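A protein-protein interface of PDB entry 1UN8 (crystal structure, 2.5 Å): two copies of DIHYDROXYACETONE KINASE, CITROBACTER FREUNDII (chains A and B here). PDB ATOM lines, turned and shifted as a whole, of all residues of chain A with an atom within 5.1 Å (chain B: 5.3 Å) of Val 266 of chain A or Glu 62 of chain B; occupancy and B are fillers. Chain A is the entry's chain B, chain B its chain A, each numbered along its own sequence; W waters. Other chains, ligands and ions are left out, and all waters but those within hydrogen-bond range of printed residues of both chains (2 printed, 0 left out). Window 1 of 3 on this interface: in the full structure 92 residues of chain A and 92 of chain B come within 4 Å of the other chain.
O of Gly 60 of chain B sits at hydrogen-bond distance from N of Leu 298 of chain B, at 2.8 Å.
OG1 of Thr 296 of chain B lies within hydrogen-bond range of O of Glu 62 of chain B (2.7 Å).
OG of Ser 265 of chain A lies within hydrogen-bond range of OE1 of Glu 268 of chain A, at 2.7 Å.
The side-chain carboxylate (OE2) of Glu 62 of chain B lies within hydrogen-bond range of the backbone NH (N) of Gly 60 of chain B (3.0 Å).
Among the printed residues, pairs that only touch across the chains: Ser 265 of chain A with Leu 298 of chain B (3.5 Å), Val 266 of chain A with Glu 62 of chain B (3.4 Å), Val 266 of chain A with Pro 63 of chain B (3.9 Å), Ala 267 of chain A with Val 16 of chain B (3.5 Å), Ala 267 of chain A with Glu 62 of chain B (3.4 Å) and Ala 270 of chain A with Val 16 of chain B (3.4 Å).
Val 266 of chain A touches just these residues of chain B: Glu 62 and Pro 63.
Glu 62 of chain B touches just these residues of chain A: Val 266 and Ala 267.
Printed residues of chain A within 4 Å of Pro 63 of chain B: Val 266 (3.9 Å).
Printed residues of chain A within 4 Å of Val 16 of chain B: Ala 267 and Ala 270.
Printed residues of chain A within 4 Å of Leu 298 of chain B: Ser 265.
The nearest printed residue of chain A that does not touch Glu 62 of chain B is Ala 270 of chain A (6.0 Å).
Of the 12 printed residues of chain B, 4 touch a printed residue of chain A.
Among the printed residues, 6 pairs touch across the chains.
Among the printed residues, no Asp or Glu carboxylate lies within 4 Å of a Lys or Arg side-chain nitrogen of the other chain.
No position is printed for both chains.
Of the 6 pairs that touch across the chains among the printed residues, none has its exchanged pair printed and touching as well.
Water W1 lies within hydrogen-bond range of OE1 of Glu 62 of chain B, N of Ala 267 of chain A and OG1 of Thr 296 of chain B.
Water W2 bridges N of Val 266 of chain A (2.7 Å) and O of Leu 298 of chain B (3.1 Å).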
ATOM      1  N   VAL A 264     -20.208  28.750  34.022  1.00  0.00           N
ATOM      2  CA  VAL A 264     -19.158  29.429  33.268  1.00  0.00           C
ATOM      3  C   VAL A 264     -18.633  28.488  32.204  1.00  0.00           C
ATOM      4  O   VAL A 264     -18.511  27.290  32.442  1.00  0.00           O
ATOM      5  CB  VAL A 264     -18.007  29.841  34.176  1.00  0.00           C
ATOM      6  CG1 VAL A 264     -16.936  30.543  33.364  1.00  0.00           C
ATOM      7  CG2 VAL A 264     -18.542  30.747  35.280  1.00  0.00           C
ATOM      8  N   SER A 265     -18.337  29.019  31.024  1.00  0.00           N
ATOM      9  CA  SER A 265     -17.827  28.178  29.945  1.00  0.00           C
ATOM     10  C   SER A 265     -16.404  27.735  30.289  1.00  0.00           C
ATOM     11  O   SER A 265     -15.695  28.417  31.031  1.00  0.00           O
ATOM     12  CB  SER A 265     -17.816  28.950  28.630  1.00  0.00           C
ATOM     13  OG  SER A 265     -16.873  29.998  28.692  1.00  0.00           O
ATOM     14  N   VAL A 266     -15.990  26.595  29.753  1.00  0.00           N
ATOM     15  CA  VAL A 266     -14.650  26.099  30.016  1.00  0.00           C
ATOM     16  C   VAL A 266     -13.647  27.131  29.507  1.00  0.00           C
ATOM     17  O   VAL A 266     -12.603  27.344  30.124  1.00  0.00           O
ATOM     18  CB  VAL A 266     -14.421  24.722  29.314  1.00  0.00           C
ATOM     19  CG1 VAL A 266     -12.959  24.295  29.448  1.00  0.00           C
ATOM     20  CG2 VAL A 266     -15.338  23.657  29.937  1.00  0.00           C
ATOM     21  N   ALA A 267     -13.967  27.777  28.389  1.00  0.00           N
ATOM     22  CA  ALA A 267     -13.075  28.784  27.827  1.00  0.00           C
ATOM     23  C   ALA A 267     -12.856  29.851  28.880  1.00  0.00           C
ATOM     24  O   ALA A 267     -11.721  30.160  29.236  1.00  0.00           O
ATOM     25  CB  ALA A 267     -13.686  29.403  26.566  1.00  0.00           C
ATOM     26  N   GLU A 268     -13.958  30.403  29.386  1.00  0.00           N
ATOM     27  CA  GLU A 268     -13.902  31.439  30.412  1.00  0.00           C
ATOM     28  C   GLU A 268     -13.074  30.986  31.616  1.00  0.00           C
ATOM     29  O   GLU A 268     -12.238  31.746  32.128  1.00  0.00           O
ATOM     30  CB  GLU A 268     -15.320  31.819  30.863  1.00  0.00           C
ATOM     31  CG  GLU A 268     -16.101  32.637  29.842  1.00  0.00           C
ATOM     32  CD  GLU A 268     -17.564  32.812  30.214  1.00  0.00           C
ATOM     33  OE1 GLU A 268     -18.365  31.868  30.009  1.00  0.00           O
ATOM     34  OE2 GLU A 268     -17.917  33.892  30.728  1.00  0.00           O
ATOM     35  N   MET A 269     -13.300  29.753  32.063  1.00  0.00           N
ATOM     36  CA  MET A 269     -12.578  29.218  33.209  1.00  0.00           C
ATOM     37  C   MET A 269     -11.076  29.204  32.971  1.00  0.00           C
ATOM     38  O   MET A 269     -10.293  29.376  33.908  1.00  0.00           O
ATOM     39  CB  MET A 269     -13.068  27.810  33.528  1.00  0.00           C
ATOM     40  CG  MET A 269     -14.453  27.777  34.138  1.00  0.00           C
ATOM     41  SD  MET A 269     -14.482  28.381  35.833  1.00  0.00           S
ATOM     42  CE  MET A 269     -14.741  30.039  35.560  1.00  0.00           C
ATOM     43  N   ALA A 270     -10.680  28.996  31.720  1.00  0.00           N
ATOM     44  CA  ALA A 270      -9.269  28.984  31.357  1.00  0.00           C
ATOM     45  C   ALA A 270      -8.715  30.409  31.474  1.00  0.00           C
ATOM     46  O   ALA A 270      -7.623  30.628  32.024  1.00  0.00           O
ATOM     47  CB  ALA A 270      -9.095  28.475  29.927  1.00  0.00           C
ATOM     48  N   VAL B  16      -7.263  31.806  26.574  1.00  0.00           N
ATOM     49  CA  VAL B  16      -7.812  30.485  26.867  1.00  0.00           C
ATOM     50  C   VAL B  16      -6.692  29.455  26.780  1.00  0.00           C
ATOM     51  O   VAL B  16      -6.572  28.571  27.619  1.00  0.00           O
ATOM     52  CB  VAL B  16      -8.948  30.099  25.858  1.00  0.00           C
ATOM     53  CG1 VAL B  16      -9.260  28.613  25.944  1.00  0.00           C
ATOM     54  CG2 VAL B  16     -10.197  30.897  26.158  1.00  0.00           C
ATOM     55  N   SER B  59     -12.730  28.259  18.028  1.00  0.00           N
ATOM     56  CA  SER B  59     -12.695  28.009  19.466  1.00  0.00           C
ATOM     57  C   SER B  59     -14.079  28.177  20.106  1.00  0.00           C
ATOM     58  O   SER B  59     -15.028  28.627  19.465  1.00  0.00           O
ATOM     59  CB  SER B  59     -11.689  28.948  20.136  1.00  0.00           C
ATOM     60  OG  SER B  59     -10.398  28.766  19.583  1.00  0.00           O
ATOM     61  N   GLY B  60     -14.182  27.821  21.378  1.00  0.00           N
ATOM     62  CA  GLY B  60     -15.450  27.923  22.065  1.00  0.00           C
ATOM     63  C   GLY B  60     -16.006  26.538  22.339  1.00  0.00           C
ATOM     64  O   GLY B  60     -17.145  26.402  22.791  1.00  0.00           O
ATOM     65  N   HIS B  61     -15.133  25.501  22.211  1.00  0.00           N
ATOM     66  CA  HIS B  61     -15.599  24.127  22.415  1.00  0.00           C
ATOM     67  C   HIS B  61     -14.672  23.457  23.386  1.00  0.00           C
ATOM     68  O   HIS B  61     -14.675  22.228  23.476  1.00  0.00           O
ATOM     69  CB  HIS B  61     -15.643  23.277  21.127  1.00  0.00           C
ATOM     70  CG  HIS B  61     -16.275  23.960  19.961  1.00  0.00           C
ATOM     71  ND1 HIS B  61     -17.572  24.428  19.991  1.00  0.00           N
ATOM     72  CD2 HIS B  61     -15.793  24.255  18.729  1.00  0.00           C
ATOM     73  CE1 HIS B  61     -17.868  24.981  18.826  1.00  0.00           C
ATOM     74  NE2 HIS B  61     -16.806  24.893  18.043  1.00  0.00           N
ATOM     75  N   GLU B  62     -13.880  24.264  24.099  1.00  0.00           N
ATOM     76  CA  GLU B  62     -12.953  23.773  25.105  1.00  0.00           C
ATOM     77  C   GLU B  62     -13.704  22.837  26.047  1.00  0.00           C
ATOM     78  O   GLU B  62     -14.891  23.094  26.355  1.00  0.00           O
ATOM     79  CB  GLU B  62     -12.416  24.951  25.904  1.00  0.00           C
ATOM     80  CG  GLU B  62     -11.603  25.937  25.087  1.00  0.00           C
ATOM     81  CD  GLU B  62     -12.453  26.790  24.163  1.00  0.00           C
ATOM     82  OE1 GLU B  62     -13.667  26.861  24.377  1.00  0.00           O
ATOM     83  OE2 GLU B  62     -11.900  27.397  23.213  1.00  0.00           O
ATOM     84  N   PRO B  63     -13.059  21.767  26.525  1.00  0.00           N
ATOM     85  CA  PRO B  63     -11.655  21.418  26.246  1.00  0.00           C
ATOM     86  C   PRO B  63     -11.224  20.969  24.840  1.00  0.00           C
ATOM     87  O   PRO B  63     -10.014  20.720  24.657  1.00  0.00           O
ATOM     88  CB  PRO B  63     -11.375  20.274  27.234  1.00  0.00           C
ATOM     89  CG  PRO B  63     -12.723  19.644  27.425  1.00  0.00           C
ATOM     90  CD  PRO B  63     -13.699  20.791  27.421  1.00  0.00           C
ATOM     91  N   ALA B  64     -12.130  20.857  23.877  1.00  0.00           N
ATOM     92  CA  ALA B  64     -11.704  20.492  22.522  1.00  0.00           C
ATOM     93  C   ALA B  64     -11.043  21.720  21.937  1.00  0.00           C
ATOM     94  O   ALA B  64     -11.543  22.814  22.143  1.00  0.00           O
ATOM     95  CB  ALA B  64     -12.902  20.105  21.678  1.00  0.00           C
ATOM     96  N   SER B 293     -17.922  17.813  30.404  1.00  0.00           N
ATOM     97  CA  SER B 293     -17.877  18.846  29.384  1.00  0.00           C
ATOM     98  C   SER B 293     -16.689  18.486  28.513  1.00  0.00           C
ATOM     99  O   SER B 293     -15.556  18.753  28.884  1.00  0.00           O
ATOM    100  CB  SER B 293     -17.677  20.221  30.023  1.00  0.00           C
ATOM    101  OG  SER B 293     -18.771  20.556  30.867  1.00  0.00           O
ATOM    102  N   LEU B 294     -16.950  17.867  27.361  1.00  0.00           N
ATOM    103  CA  LEU B 294     -15.888  17.426  26.454  1.00  0.00           C
ATOM    104  C   LEU B 294     -15.772  18.243  25.167  1.00  0.00           C
ATOM    105  O   LEU B 294     -14.673  18.652  24.785  1.00  0.00           O
ATOM    106  CB  LEU B 294     -16.101  15.950  26.140  1.00  0.00           C
ATOM    107  CG  LEU B 294     -16.078  15.100  27.412  1.00  0.00           C
ATOM    108  CD1 LEU B 294     -16.487  13.677  27.108  1.00  0.00           C
ATOM    109  CD2 LEU B 294     -14.684  15.151  28.009  1.00  0.00           C
ATOM    110  N   VAL B 295     -16.893  18.463  24.491  1.00  0.00           N
ATOM    111  CA  VAL B 295     -16.914  19.268  23.271  1.00  0.00           C
ATOM    112  C   VAL B 295     -18.074  20.225  23.538  1.00  0.00           C
ATOM    113  O   VAL B 295     -19.250  19.852  23.413  1.00  0.00           O
ATOM    114  CB  VAL B 295     -17.208  18.410  22.016  1.00  0.00           C
ATOM    115  CG1 VAL B 295     -17.297  19.296  20.795  1.00  0.00           C
ATOM    116  CG2 VAL B 295     -16.112  17.371  21.814  1.00  0.00           C
ATOM    117  N   THR B 296     -17.740  21.453  23.924  1.00  0.00           N
ATOM    118  CA  THR B 296     -18.754  22.431  24.281  1.00  0.00           C
ATOM    119  C   THR B 296     -19.111  23.458  23.243  1.00  0.00           C
ATOM    120  O   THR B 296     -18.559  23.481  22.153  1.00  0.00           O
ATOM    121  CB  THR B 296     -18.350  23.207  25.538  1.00  0.00           C
ATOM    122  OG1 THR B 296     -17.169  23.967  25.258  1.00  0.00           O
ATOM    123  CG2 THR B 296     -18.097  22.254  26.703  1.00  0.00           C
ATOM    124  N   LEU B 298     -19.458  26.927  24.315  1.00  0.00           N
ATOM    125  CA  LEU B 298     -19.345  27.938  25.345  1.00  0.00           C
ATOM    126  C   LEU B 298     -20.237  27.492  26.509  1.00  0.00           C
ATOM    127  O   LEU B 298     -20.099  26.360  26.975  1.00  0.00           O
ATOM    128  CB  LEU B 298     -19.753  29.304  24.794  1.00  0.00           C
ATOM    129  CG  LEU B 298     -18.726  29.821  23.776  1.00  0.00           C
ATOM    130  CD1 LEU B 298     -19.172  31.127  23.150  1.00  0.00           C
ATOM    131  CD2 LEU B 298     -17.404  30.003  24.483  1.00  0.00           C
HETATM  132  O   HOH W   1     -15.740  26.785  26.015  1.00  0.00           O
HETATM  133  O   HOH W   2     -17.964  25.103  28.783  1.00  0.00           O
